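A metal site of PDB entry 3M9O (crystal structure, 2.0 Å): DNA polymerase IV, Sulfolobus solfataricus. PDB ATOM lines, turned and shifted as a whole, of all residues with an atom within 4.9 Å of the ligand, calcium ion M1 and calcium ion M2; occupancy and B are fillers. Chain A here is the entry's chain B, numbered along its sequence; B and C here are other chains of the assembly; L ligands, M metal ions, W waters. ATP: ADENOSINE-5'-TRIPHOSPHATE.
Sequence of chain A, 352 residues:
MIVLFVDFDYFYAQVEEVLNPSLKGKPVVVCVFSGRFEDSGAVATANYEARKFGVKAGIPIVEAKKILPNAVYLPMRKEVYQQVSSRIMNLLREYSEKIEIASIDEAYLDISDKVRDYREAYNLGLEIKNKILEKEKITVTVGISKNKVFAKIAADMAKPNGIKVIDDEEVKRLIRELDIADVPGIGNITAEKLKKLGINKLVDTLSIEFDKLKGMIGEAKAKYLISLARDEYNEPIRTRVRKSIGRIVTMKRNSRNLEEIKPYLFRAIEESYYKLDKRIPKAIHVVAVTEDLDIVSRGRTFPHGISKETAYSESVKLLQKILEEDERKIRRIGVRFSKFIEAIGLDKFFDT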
ATOM      1  N   PHE A   5       9.148   3.579 -18.253  1.00  0.00           N
ATOM      2  CA  PHE A   5       7.745   3.437 -17.917  1.00  0.00           C
ATOM      3  C   PHE A   5       7.622   2.717 -16.591  1.00  0.00           C
ATOM      4  O   PHE A   5       8.304   1.700 -16.367  1.00  0.00           O
ATOM      5  CB  PHE A   5       7.055   2.640 -19.039  1.00  0.00           C
ATOM      6  CG  PHE A   5       5.632   2.289 -18.763  1.00  0.00           C
ATOM      7  CD1 PHE A   5       4.632   3.261 -18.763  1.00  0.00           C
ATOM      8  CD2 PHE A   5       5.263   0.953 -18.581  1.00  0.00           C
ATOM      9  CE1 PHE A   5       3.299   2.918 -18.589  1.00  0.00           C
ATOM     10  CE2 PHE A   5       3.922   0.566 -18.400  1.00  0.00           C
ATOM     11  CZ  PHE A   5       2.934   1.562 -18.415  1.00  0.00           C
ATOM     12  N   ASP A   7       4.867   0.960 -13.890  1.00  0.00           N
ATOM     13  CA  ASP A   7       3.522   0.418 -13.811  1.00  0.00           C
ATOM     14  C   ASP A   7       3.423  -0.292 -12.460  1.00  0.00           C
ATOM     15  O   ASP A   7       4.078  -1.308 -12.261  1.00  0.00           O
ATOM     16  CB  ASP A   7       3.365  -0.559 -14.955  1.00  0.00           C
ATOM     17  CG  ASP A   7       1.988  -1.153 -15.027  1.00  0.00           C
ATOM     18  OD1 ASP A   7       1.390  -1.364 -13.992  1.00  0.00           O
ATOM     19  OD2 ASP A   7       1.497  -1.421 -16.136  1.00  0.00           O
ATOM     20  N   PHE A   8       2.649   0.253 -11.521  1.00  0.00           N
ATOM     21  CA  PHE A   8       2.540  -0.335 -10.164  1.00  0.00           C
ATOM     22  C   PHE A   8       1.908  -1.753 -10.195  1.00  0.00           C
ATOM     23  O   PHE A   8       0.874  -1.978 -10.860  1.00  0.00           O
ATOM     24  CB  PHE A   8       1.688   0.563  -9.237  1.00  0.00           C
ATOM     25  CG  PHE A   8       1.976   2.058  -9.352  1.00  0.00           C
ATOM     26  CD1 PHE A   8       3.161   2.520  -9.872  1.00  0.00           C
ATOM     27  CD2 PHE A   8       1.064   2.988  -8.859  1.00  0.00           C
ATOM     28  CE1 PHE A   8       3.463   3.921  -9.905  1.00  0.00           C
ATOM     29  CE2 PHE A   8       1.341   4.361  -8.894  1.00  0.00           C
ATOM     30  CZ  PHE A   8       2.536   4.826  -9.416  1.00  0.00           C
ATOM     31  N   ASP A   9       2.488  -2.708  -9.444  1.00  0.00           N
ATOM     32  CA  ASP A   9       1.927  -4.070  -9.425  1.00  0.00           C
ATOM     33  C   ASP A   9       0.600  -4.209  -8.642  1.00  0.00           C
ATOM     34  O   ASP A   9       0.470  -3.655  -7.578  1.00  0.00           O
ATOM     35  CB  ASP A   9       2.959  -5.050  -8.813  1.00  0.00           C
ATOM     36  CG  ASP A   9       4.260  -5.074  -9.580  1.00  0.00           C
ATOM     37  OD1 ASP A   9       4.208  -5.070 -10.856  1.00  0.00           O
ATOM     38  OD2 ASP A   9       5.341  -5.077  -8.935  1.00  0.00           O
ATOM     39  N   TYR A  10      -0.334  -5.021  -9.156  1.00  0.00           N
ATOM     40  CA  TYR A  10      -1.653  -5.275  -8.554  1.00  0.00           C
ATOM     41  C   TYR A  10      -2.069  -4.147  -7.633  1.00  0.00           C
ATOM     42  O   TYR A  10      -2.583  -4.371  -6.531  1.00  0.00           O
ATOM     43  CB  TYR A  10      -1.668  -6.611  -7.785  1.00  0.00           C
ATOM     44  CG  TYR A  10      -0.653  -6.828  -6.686  1.00  0.00           C
ATOM     45  CD1 TYR A  10       0.701  -7.074  -7.001  1.00  0.00           C
ATOM     46  CD2 TYR A  10      -1.052  -6.925  -5.316  1.00  0.00           C
ATOM     47  CE1 TYR A  10       1.632  -7.425  -5.960  1.00  0.00           C
ATOM     48  CE2 TYR A  10      -0.130  -7.270  -4.304  1.00  0.00           C
ATOM     49  CZ  TYR A  10       1.180  -7.507  -4.611  1.00  0.00           C
ATOM     50  OH  TYR A  10       2.099  -7.770  -3.610  1.00  0.00           O
ATOM     51  N   PHE A  11      -1.944  -2.941  -8.181  1.00  0.00           N
ATOM     52  CA  PHE A  11      -2.148  -1.752  -7.414  1.00  0.00           C
ATOM     53  C   PHE A  11      -3.221  -1.713  -6.346  1.00  0.00           C
ATOM     54  O   PHE A  11      -2.880  -1.600  -5.196  1.00  0.00           O
ATOM     55  CB  PHE A  11      -2.273  -0.542  -8.333  1.00  0.00           C
ATOM     56  CG  PHE A  11      -2.064   0.774  -7.606  1.00  0.00           C
ATOM     57  CD1 PHE A  11      -1.004   0.962  -6.704  1.00  0.00           C
ATOM     58  CD2 PHE A  11      -2.970   1.822  -7.798  1.00  0.00           C
ATOM     59  CE1 PHE A  11      -0.861   2.142  -6.006  1.00  0.00           C
ATOM     60  CE2 PHE A  11      -2.827   3.002  -7.101  1.00  0.00           C
ATOM     61  CZ  PHE A  11      -1.776   3.176  -6.206  1.00  0.00           C
ATOM     62  N   TYR A  12      -4.506  -1.800  -6.701  1.00  0.00           N
ATOM     63  CA  TYR A  12      -5.539  -1.709  -5.669  1.00  0.00           C
ATOM     64  C   TYR A  12      -5.375  -2.768  -4.551  1.00  0.00           C
ATOM     65  O   TYR A  12      -5.496  -2.461  -3.333  1.00  0.00           O
ATOM     66  CB  TYR A  12      -6.927  -1.854  -6.252  1.00  0.00           C
ATOM     67  CG  TYR A  12      -7.393  -0.661  -7.058  1.00  0.00           C
ATOM     68  CD1 TYR A  12      -6.517   0.359  -7.436  1.00  0.00           C
ATOM     69  CD2 TYR A  12      -8.703  -0.597  -7.521  1.00  0.00           C
ATOM     70  CE1 TYR A  12      -6.933   1.409  -8.243  1.00  0.00           C
ATOM     71  CE2 TYR A  12      -9.130   0.420  -8.322  1.00  0.00           C
ATOM     72  CZ  TYR A  12      -8.249   1.431  -8.689  1.00  0.00           C
ATOM     73  OH  TYR A  12      -8.695   2.462  -9.508  1.00  0.00           O
ATOM     74  N   VAL A  32     -16.168  -3.864  -6.828  1.00  0.00           N
ATOM     75  CA  VAL A  32     -16.920  -2.669  -7.185  1.00  0.00           C
ATOM     76  C   VAL A  32     -18.359  -3.164  -7.093  1.00  0.00           C
ATOM     77  O   VAL A  32     -18.914  -3.689  -8.052  1.00  0.00           O
ATOM     78  CB  VAL A  32     -16.645  -2.194  -8.602  1.00  0.00           C
ATOM     79  CG1 VAL A  32     -17.483  -0.935  -8.889  1.00  0.00           C
ATOM     80  CG2 VAL A  32     -15.159  -1.900  -8.769  1.00  0.00           C
ATOM     81  N   VAL A  43     -15.183  -7.245 -10.331  1.00  0.00           N
ATOM     82  CA  VAL A  43     -13.875  -7.173  -9.722  1.00  0.00           C
ATOM     83  C   VAL A  43     -13.093  -6.010 -10.326  1.00  0.00           C
ATOM     84  O   VAL A  43     -13.013  -5.890 -11.542  1.00  0.00           O
ATOM     85  CB  VAL A  43     -13.090  -8.497  -9.951  1.00  0.00           C
ATOM     86  CG1 VAL A  43     -11.690  -8.345  -9.444  1.00  0.00           C
ATOM     87  CG2 VAL A  43     -13.784  -9.655  -9.191  1.00  0.00           C
ATOM     88  N   ALA A  44     -12.535  -5.138  -9.496  1.00  0.00           N
ATOM     89  CA  ALA A  44     -11.696  -4.044  -9.989  1.00  0.00           C
ATOM     90  C   ALA A  44     -10.293  -4.619 -10.290  1.00  0.00           C
ATOM     91  O   ALA A  44      -9.653  -4.280 -11.320  1.00  0.00           O
ATOM     92  CB  ALA A  44     -11.581  -2.961  -8.943  1.00  0.00           C
ATOM     93  N   THR A  45      -9.804  -5.453  -9.382  1.00  0.00           N
ATOM     94  CA  THR A  45      -8.535  -6.120  -9.551  1.00  0.00           C
ATOM     95  C   THR A  45      -8.354  -7.162  -8.429  1.00  0.00           C
ATOM     96  O   THR A  45      -9.133  -7.224  -7.490  1.00  0.00           O
ATOM     97  CB  THR A  45      -7.371  -5.131  -9.519  1.00  0.00           C
ATOM     98  OG1 THR A  45      -6.225  -5.769 -10.079  1.00  0.00           O
ATOM     99  CG2 THR A  45      -7.064  -4.676  -8.120  1.00  0.00           C
ATOM    100  N   ALA A  46      -7.325  -7.988  -8.538  1.00  0.00           N
ATOM    101  CA  ALA A  46      -7.039  -8.999  -7.524  1.00  0.00           C
ATOM    102  C   ALA A  46      -5.547  -9.213  -7.531  1.00  0.00           C
ATOM    103  O   ALA A  46      -4.901  -8.947  -8.573  1.00  0.00           O
ATOM    104  CB  ALA A  46      -7.732 -10.312  -7.865  1.00  0.00           C
ATOM    105  N   TYR A  48      -2.084 -11.521  -7.607  1.00  0.00           N
ATOM    106  CA  TYR A  48      -1.816 -12.755  -8.381  1.00  0.00           C
ATOM    107  C   TYR A  48      -2.224 -14.039  -7.642  1.00  0.00           C
ATOM    108  O   TYR A  48      -2.566 -15.021  -8.274  1.00  0.00           O
ATOM    109  CB  TYR A  48      -0.348 -12.785  -8.769  1.00  0.00           C
ATOM    110  CG  TYR A  48       0.071 -11.660  -9.736  1.00  0.00           C
ATOM    111  CD1 TYR A  48       0.121 -11.854 -11.120  1.00  0.00           C
ATOM    112  CD2 TYR A  48       0.439 -10.431  -9.245  1.00  0.00           C
ATOM    113  CE1 TYR A  48       0.538 -10.826 -11.981  1.00  0.00           C
ATOM    114  CE2 TYR A  48       0.833  -9.415 -10.038  1.00  0.00           C
ATOM    115  CZ  TYR A  48       0.903  -9.591 -11.408  1.00  0.00           C
ATOM    116  OH  TYR A  48       1.344  -8.544 -12.236  1.00  0.00           O
ATOM    117  N   ARG A  51      -5.478 -14.010  -8.970  1.00  0.00           N
ATOM    118  CA  ARG A  51      -5.461 -13.989 -10.427  1.00  0.00           C
ATOM    119  C   ARG A  51      -4.976 -15.274 -11.064  1.00  0.00           C
ATOM    120  O   ARG A  51      -5.459 -15.651 -12.129  1.00  0.00           O
ATOM    121  CB  ARG A  51      -4.556 -12.845 -10.940  1.00  0.00           C
ATOM    122  CG  ARG A  51      -5.140 -11.492 -10.684  1.00  0.00           C
ATOM    123  CD  ARG A  51      -5.153 -10.694 -11.962  1.00  0.00           C
ATOM    124  NE  ARG A  51      -4.862  -9.309 -11.610  1.00  0.00           N
ATOM    125  CZ  ARG A  51      -3.686  -8.740 -11.782  1.00  0.00           C
ATOM    126  NH1 ARG A  51      -2.682  -9.418 -12.317  1.00  0.00           N
ATOM    127  NH2 ARG A  51      -3.509  -7.499 -11.367  1.00  0.00           N
ATOM    128  N   ALA A  57      -9.712  -8.521 -13.055  1.00  0.00           N
ATOM    129  CA  ALA A  57     -10.479  -7.313 -13.328  1.00  0.00           C
ATOM    130  C   ALA A  57     -11.590  -7.524 -14.340  1.00  0.00           C
ATOM    131  O   ALA A  57     -11.390  -8.111 -15.413  1.00  0.00           O
ATOM    132  CB  ALA A  57      -9.520  -6.206 -13.837  1.00  0.00           C
ATOM    133  N   GLY A  58     -12.789  -7.093 -13.968  1.00  0.00           N
ATOM    134  CA  GLY A  58     -13.878  -7.209 -14.915  1.00  0.00           C
ATOM    135  C   GLY A  58     -14.835  -8.364 -14.760  1.00  0.00           C
ATOM    136  O   GLY A  58     -15.951  -8.263 -15.216  1.00  0.00           O
ATOM    137  N   ILE A 104      -3.982   6.010 -13.188  1.00  0.00           N
ATOM    138  CA  ILE A 104      -3.804   5.930 -11.742  1.00  0.00           C
ATOM    139  C   ILE A 104      -2.533   5.204 -11.306  1.00  0.00           C
ATOM    140  O   ILE A 104      -2.039   5.421 -10.201  1.00  0.00           O
ATOM    141  CB  ILE A 104      -5.029   5.268 -11.084  1.00  0.00           C
ATOM    142  CG1 ILE A 104      -5.016   5.554  -9.551  1.00  0.00           C
ATOM    143  CG2 ILE A 104      -5.034   3.760 -11.396  1.00  0.00           C
ATOM    144  CD1 ILE A 104      -6.336   5.715  -8.974  1.00  0.00           C
ATOM    145  N   ASP A 105      -1.981   4.340 -12.157  1.00  0.00           N
ATOM    146  CA  ASP A 105      -0.780   3.633 -11.771  1.00  0.00           C
ATOM    147  C   ASP A 105       0.309   3.481 -12.858  1.00  0.00           C
ATOM    148  O   ASP A 105       1.090   2.520 -12.826  1.00  0.00           O
ATOM    149  CB  ASP A 105      -1.217   2.260 -11.251  1.00  0.00           C
ATOM    150  CG  ASP A 105      -1.467   1.289 -12.377  1.00  0.00           C
ATOM    151  OD1 ASP A 105      -1.833   1.691 -13.530  1.00  0.00           O
ATOM    152  OD2 ASP A 105      -1.302   0.074 -12.093  1.00  0.00           O
ATOM    153  N   GLU A 106       0.358   4.416 -13.807  1.00  0.00           N
ATOM    154  CA  GLU A 106       1.357   4.365 -14.888  1.00  0.00           C
ATOM    155  C   GLU A 106       1.927   5.734 -15.126  1.00  0.00           C
ATOM    156  O   GLU A 106       1.218   6.755 -15.057  1.00  0.00           O
ATOM    157  CB  GLU A 106       0.725   3.925 -16.203  1.00  0.00           C
ATOM    158  CG  GLU A 106       0.070   2.587 -16.199  1.00  0.00           C
ATOM    159  CD  GLU A 106      -0.696   2.393 -17.479  1.00  0.00           C
ATOM    160  OE1 GLU A 106      -1.593   3.230 -17.738  1.00  0.00           O
ATOM    161  OE2 GLU A 106      -0.383   1.427 -18.205  1.00  0.00           O
ATOM    162  N   LYS A 152       6.362   0.323 -22.735  1.00  0.00           N
ATOM    163  CA  LYS A 152       5.188  -0.338 -22.129  1.00  0.00           C
ATOM    164  C   LYS A 152       5.249  -1.863 -22.369  1.00  0.00           C
ATOM    165  O   LYS A 152       4.981  -2.636 -21.479  1.00  0.00           O
ATOM    166  CB  LYS A 152       3.912   0.216 -22.736  1.00  0.00           C
ATOM    167  CG  LYS A 152       2.595  -0.305 -22.079  1.00  0.00           C
ATOM    168  CD  LYS A 152       1.379   0.358 -22.713  1.00  0.00           C
ATOM    169  CE  LYS A 152       0.085  -0.052 -22.054  1.00  0.00           C
ATOM    170  NZ  LYS A 152      -0.004   0.445 -20.662  1.00  0.00           N
ATOM    171  N   LYS A 159       6.438  -7.769 -15.662  1.00  0.00           N
ATOM    172  CA  LYS A 159       5.634  -7.734 -14.453  1.00  0.00           C
ATOM    173  C   LYS A 159       5.323  -9.117 -13.864  1.00  0.00           C
ATOM    174  O   LYS A 159       5.221 -10.120 -14.584  1.00  0.00           O
ATOM    175  CB  LYS A 159       4.343  -6.893 -14.664  1.00  0.00           C
ATOM    176  CG  LYS A 159       3.446  -7.311 -15.773  1.00  0.00           C
ATOM    177  CD  LYS A 159       2.125  -6.502 -15.747  1.00  0.00           C
ATOM    178  CE  LYS A 159       2.357  -5.014 -16.014  1.00  0.00           C
ATOM    179  NZ  LYS A 159       1.056  -4.254 -16.140  1.00  0.00           N
ATOM    180  P    DC B  12      -5.688  -1.948 -25.781  1.00  0.00           P
ATOM    181  OP1  DC B  12      -4.289  -2.250 -26.190  1.00  0.00           O
ATOM    182  OP2  DC B  12      -6.653  -3.073 -25.629  1.00  0.00           O
ATOM    183  O5'  DC B  12      -5.681  -1.153 -24.407  1.00  0.00           O
ATOM    184  C5'  DC B  12      -4.847  -0.007 -24.329  1.00  0.00           C
ATOM    185  C4'  DC B  12      -5.090   0.598 -22.972  1.00  0.00           C
ATOM    186  O4'  DC B  12      -6.466   1.029 -22.893  1.00  0.00           O
ATOM    187  C3'  DC B  12      -4.907  -0.466 -21.867  1.00  0.00           C
ATOM    188  O3'  DC B  12      -3.886  -0.090 -20.953  1.00  0.00           O
ATOM    189  C2'  DC B  12      -6.271  -0.561 -21.186  1.00  0.00           C
ATOM    190  C1'  DC B  12      -6.958   0.733 -21.601  1.00  0.00           C
ATOM    191  N1   DC B  12      -8.400   0.518 -21.649  1.00  0.00           N
ATOM    192  C2   DC B  12      -9.202   1.405 -20.925  1.00  0.00           C
ATOM    193  O2   DC B  12      -8.666   2.374 -20.382  1.00  0.00           O
ATOM    194  N3   DC B  12     -10.526   1.182 -20.842  1.00  0.00           N
ATOM    195  C4   DC B  12     -11.073   0.141 -21.465  1.00  0.00           C
ATOM    196  N4   DC B  12     -12.386  -0.024 -21.361  1.00  0.00           N
ATOM    197  C5   DC B  12     -10.291  -0.785 -22.231  1.00  0.00           C
ATOM    198  C6   DC B  12      -8.973  -0.544 -22.316  1.00  0.00           C
ATOM    199  P    DC B  13      -3.671  -0.981 -19.610  1.00  0.00           P
ATOM    200  OP1  DC B  13      -2.244  -0.996 -19.354  1.00  0.00           O
ATOM    201  OP2  DC B  13      -4.369  -2.303 -19.764  1.00  0.00           O
ATOM    202  O5'  DC B  13      -4.468  -0.189 -18.484  1.00  0.00           O
ATOM    203  C5'  DC B  13      -4.090   1.179 -18.282  1.00  0.00           C
ATOM    204  C4'  DC B  13      -4.862   1.763 -17.112  1.00  0.00           C
ATOM    205  O4'  DC B  13      -6.246   1.937 -17.492  1.00  0.00           O
ATOM    206  C3'  DC B  13      -4.829   0.909 -15.820  1.00  0.00           C
ATOM    207  C2'  DC B  13      -6.276   0.816 -15.348  1.00  0.00           C
ATOM    208  C1'  DC B  13      -7.105   1.614 -16.388  1.00  0.00           C
ATOM    209  N1   DC B  13      -8.172   0.743 -16.898  1.00  0.00           N
ATOM    210  C2   DC B  13      -9.403   0.919 -16.331  1.00  0.00           C
ATOM    211  O2   DC B  13      -9.517   1.758 -15.412  1.00  0.00           O
ATOM    212  N3   DC B  13     -10.437   0.188 -16.774  1.00  0.00           N
ATOM    213  C4   DC B  13     -10.274  -0.714 -17.736  1.00  0.00           C
ATOM    214  N4   DC B  13     -11.326  -1.415 -18.127  1.00  0.00           N
ATOM    215  C5   DC B  13      -9.006  -0.944 -18.344  1.00  0.00           C
ATOM    216  C6   DC B  13      -7.984  -0.195 -17.891  1.00  0.00           C
ATOM    217  P    DT C   3     -21.588  -3.494 -14.842  1.00  0.00           P
ATOM    218  OP1  DT C   3     -23.029  -3.720 -14.498  1.00  0.00           O
ATOM    219  OP2  DT C   3     -21.227  -2.664 -16.026  1.00  0.00           O
ATOM    220  O5'  DT C   3     -20.852  -2.943 -13.543  1.00  0.00           O
ATOM    221  C5'  DT C   3     -21.139  -3.471 -12.240  1.00  0.00           C
ATOM    222  C4'  DT C   3     -20.462  -2.553 -11.256  1.00  0.00           C
ATOM    223  O4'  DT C   3     -19.028  -2.730 -11.380  1.00  0.00           O
ATOM    224  C3'  DT C   3     -20.710  -1.085 -11.598  1.00  0.00           C
ATOM    225  O3'  DT C   3     -20.621  -0.291 -10.415  1.00  0.00           O
ATOM    226  C2'  DT C   3     -19.557  -0.757 -12.536  1.00  0.00           C
ATOM    227  C1'  DT C   3     -18.419  -1.558 -11.898  1.00  0.00           C
ATOM    228  N1   DT C   3     -17.412  -2.006 -12.866  1.00  0.00           N
ATOM    229  C2   DT C   3     -16.098  -1.593 -12.726  1.00  0.00           C
ATOM    230  O2   DT C   3     -15.690  -0.815 -11.874  1.00  0.00           O
ATOM    231  N3   DT C   3     -15.260  -2.129 -13.658  1.00  0.00           N
ATOM    232  C4   DT C   3     -15.573  -3.006 -14.671  1.00  0.00           C
ATOM    233  O4   DT C   3     -14.695  -3.432 -15.400  1.00  0.00           O
ATOM    234  C5   DT C   3     -16.951  -3.371 -14.753  1.00  0.00           C
ATOM    235  C7   DT C   3     -17.383  -4.329 -15.823  1.00  0.00           C
ATOM    236  C6   DT C   3     -17.795  -2.851 -13.869  1.00  0.00           C
ATOM    237  P    DG C   4     -21.351   1.139 -10.366  1.00  0.00           P
ATOM    238  OP1  DG C   4     -21.789   1.498  -9.038  1.00  0.00           O
ATOM    239  OP2  DG C   4     -22.312   1.367 -11.405  1.00  0.00           O
ATOM    240  O5'  DG C   4     -20.149   2.070 -10.417  1.00  0.00           O
ATOM    241  C5'  DG C   4     -19.449   2.067 -11.496  1.00  0.00           C
ATOM    242  C4'  DG C   4     -18.109   2.715 -11.248  1.00  0.00           C
ATOM    243  O4'  DG C   4     -17.150   1.859 -11.905  1.00  0.00           O
ATOM    244  C3'  DG C   4     -18.166   4.096 -11.824  1.00  0.00           C
ATOM    245  O3'  DG C   4     -17.371   5.065 -11.179  1.00  0.00           O
ATOM    246  C2'  DG C   4     -17.798   3.679 -13.243  1.00  0.00           C
ATOM    247  C1'  DG C   4     -16.738   2.498 -12.919  1.00  0.00           C
ATOM    248  N9   DG C   4     -16.407   1.707 -14.167  1.00  0.00           N
ATOM    249  C8   DG C   4     -17.238   1.311 -15.241  1.00  0.00           C
ATOM    250  N7   DG C   4     -16.621   0.695 -16.252  1.00  0.00           N
ATOM    251  C5   DG C   4     -15.248   0.703 -15.750  1.00  0.00           C
ATOM    252  C6   DG C   4     -14.024   0.195 -16.281  1.00  0.00           C
ATOM    253  O6   DG C   4     -13.870  -0.392 -17.325  1.00  0.00           O
ATOM    254  N1   DG C   4     -12.892   0.451 -15.444  1.00  0.00           N
ATOM    255  C2   DG C   4     -12.930   1.105 -14.238  1.00  0.00           C
ATOM    256  N2   DG C   4     -11.773   1.260 -13.589  1.00  0.00           N
ATOM    257  N3   DG C   4     -14.047   1.560 -13.722  1.00  0.00           N
ATOM    258  C4   DG C   4     -15.153   1.336 -14.506  1.00  0.00           C
HETATM  259  PG  ATP L   1      -0.838  -5.527 -12.979  1.00  0.00           P
HETATM  260  O1G ATP L   1      -1.065  -6.284 -14.385  1.00  0.00           O
HETATM  261  O2G ATP L   1      -0.070  -6.337 -11.853  1.00  0.00           O
HETATM  262  O3G ATP L   1      -0.158  -4.190 -13.235  1.00  0.00           O
HETATM  263  PB  ATP L   1      -3.166  -4.204 -11.643  1.00  0.00           P
HETATM  264  O1B ATP L   1      -4.022  -4.713 -10.515  1.00  0.00           O
HETATM  265  O2B ATP L   1      -2.213  -3.027 -11.347  1.00  0.00           O
HETATM  266  O3B ATP L   1      -2.430  -5.395 -12.415  1.00  0.00           O
HETATM  267  PA  ATP L   1      -3.896  -2.848 -14.116  1.00  0.00           P
HETATM  268  O1A ATP L   1      -2.493  -2.507 -14.180  1.00  0.00           O
HETATM  269  O2A ATP L   1      -4.594  -3.504 -15.286  1.00  0.00           O
HETATM  270  O3A ATP L   1      -4.198  -3.734 -12.793  1.00  0.00           O
HETATM  271  O5' ATP L   1      -4.687  -1.536 -13.750  1.00  0.00           O
HETATM  272  C5' ATP L   1      -4.281  -0.741 -12.663  1.00  0.00           C
HETATM  273  C4' ATP L   1      -5.350  -0.554 -11.586  1.00  0.00           C
HETATM  274  O4' ATP L   1      -6.523   0.059 -12.098  1.00  0.00           O
HETATM  275  C3' ATP L   1      -5.785  -1.811 -10.793  1.00  0.00           C
HETATM  276  O3' ATP L   1      -5.295  -1.927  -9.508  1.00  0.00           O
HETATM  277  C2' ATP L   1      -7.282  -1.821 -10.837  1.00  0.00           C
HETATM  278  C1' ATP L   1      -7.727  -0.626 -11.689  1.00  0.00           C
HETATM  279  N9  ATP L   1      -8.508  -1.270 -12.792  1.00  0.00           N
HETATM  280  C8  ATP L   1      -8.007  -1.885 -13.882  1.00  0.00           C
HETATM  281  N7  ATP L   1      -8.980  -2.401 -14.623  1.00  0.00           N
HETATM  282  C5  ATP L   1     -10.158  -2.125 -14.029  1.00  0.00           C
HETATM  283  C6  ATP L   1     -11.602  -2.427 -14.271  1.00  0.00           C
HETATM  284  N6  ATP L   1     -11.990  -3.145 -15.372  1.00  0.00           N
HETATM  285  N1  ATP L   1     -12.526  -1.949 -13.365  1.00  0.00           N
HETATM  286  C2  ATP L   1     -12.171  -1.262 -12.263  1.00  0.00           C
HETATM  287  N3  ATP L   1     -10.880  -0.960 -11.990  1.00  0.00           N
HETATM  288  C4  ATP L   1      -9.843  -1.388 -12.813  1.00  0.00           C
HETATM  289 CA    CA M   1      -0.556  -2.077 -12.759  1.00  0.00          CA
HETATM  290 CA    CA M   2      -0.626  -0.983 -17.523  1.00  0.00          CA
HETATM  291  O   HOH W   1       3.029  -3.940 -12.796  1.00  0.00           O
HETATM  292  O   HOH W   2      -8.627  -4.160 -16.744  1.00  0.00           O
HETATM  293  O   HOH W   3     -10.889   1.774 -10.873  1.00  0.00           O
HETATM  294  O   HOH W   4      -1.737  -0.144 -15.392  1.00  0.00           O
HETATM  295  O   HOH W   5     -10.850  -4.873 -17.636  1.00  0.00           O
HETATM  296  O   HOH W   6      -3.503  -6.022 -15.777  1.00  0.00           O
HETATM  297  O   HOH W   7       0.638  -2.302 -19.117  1.00  0.00           O
HETATM  298  O   HOH W   8      -1.647  -3.203 -16.986  1.00  0.00           O
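N4 of DC 13 of chain B sits at hydrogen-bond distance from a nitrogen (N6) of the ligand (3.3 Å).
OG1 of Thr 45 lies within hydrogen-bond range of O1B of the ligand (2.5 Å).
NH2 of Arg 51 is in salt-bridge range of O1B of the ligand, 3.0 Å away.
An oxygen (O2G) of the ligand lies within hydrogen-bond range of the side-chain hydroxyl of Tyr 48 (2.6 Å).
O4 of DT 3 of chain C lies within hydrogen-bond range of a nitrogen (N6) of the ligand, at 2.7 Å.
O3' of the ligand sits at hydrogen-bond distance from N of Tyr 12 of chain A (2.9 Å).
The backbone NH (N) of Tyr 10 is in hydrogen-bond range of an oxygen (O2G) of the ligand.
The side-chain amino group (NZ) of Lys 159 lies within salt-bridge range of an oxygen (O1G) of the ligand, at 3.4 Å.
The backbone NH of Phe 11 lies close to an oxygen (O2B) of the ligand, 3.2 Å away.
The side-chain carboxylate (OD2) of Asp 7 sits close to the side-chain amino group (NZ) of Lys 159, at 2.9 Å.
NZ of Lys 152 sits close to OP1 of DC 13 of chain B (3.0 Å).
The side-chain hydroxyl (OG1) of Thr 45 is in hydrogen-bond range of the guanidinium group (NH2) of Arg 51 (3.5 Å).
The side-chain amino group of Lys 152 sits close to the side-chain carboxylate of Glu 106 (2.7 Å).
NE of Arg 51 lies within hydrogen-bond range of O of Ala 46, 3.1 Å away.
N2 of DG 4 of chain C lies close to N3 of the ligand, 2.9 Å away.
CA of Asp 9 touches O2G of the ligand (3.9 Å).
Ala 44 touches the ligand (O to C4, 3.3 Å).
Ala 57 touches the ligand (CB to N7, 3.9 Å).
Hydrophobic or aromatic side chains that line the ligand: Phe 11, Tyr 12 of chain A, Ala 44, Tyr 48 and Ala 57.
Within 4 Å of the ligand: Asp 7, Phe 8, Asp 9, Tyr 10, Phe 11, Tyr 12 of chain A, Ala 44, Thr 45, Tyr 48, Arg 51, Ala 57, Asp 105, Lys 159, DC 13 of chain B, DT 3 of chain C and DG 4 of chain C.
The nearest printed residue that does not touch the ligand is Ile 104 (4.1 Å).
Of the 25 residues printed, 3 come within 4 Å of calcium ion M1.
Lys 152 touches calcium ion M2 (NZ to CA, 3.5 Å).
Lys 159 touches calcium ion M2 (NZ to CA, 3.9 Å).
Along chain A the residues within 4 Å of calcium ion M2 span positions 7 to 159.
The nearest printed residue that does not touch calcium ion M2 is Phe 5 (4.5 Å).
Calcium ion M1 is bound by an oxygen (O3G) of the ligand (2.2 Å), the side-chain carboxylate of Asp 105 (2.4 Å), an oxygen (O2B) of the ligand (2.4 Å), the backbone carbonyl oxygen of Phe 8 (2.4 Å), the side-chain carboxylate of Asp 7 (2.4 Å) and an oxygen (O1A) of the ligand (2.4 Å).
Water W7 is bound to calcium ion M2 (2.4 Å).
OP1 of DC 13 of chain B is bound to calcium ion M2 (2.4 Å).
Water W8 is bound to calcium ion M2 (2.5 Å).
OE2 of Glu 106 binds calcium ion M2 (2.5 Å).
Water W4 binds calcium ion M2, at 2.5 Å.
OD2 of Asp 7 is bound to calcium ion M2 (2.6 Å).
Calcium ion M2 has six donor atoms within binding distance.
Water W8 bridges NZ of Lys 159 and O2A of the ligand.
Water W3 lies within hydrogen-bond range of OH of Tyr 12 of chain A, N2 of DG 4 of chain C and N3 of the ligand.
Water W1 lies within hydrogen-bond range of OD1 of Asp 9 and O of Asp 7.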
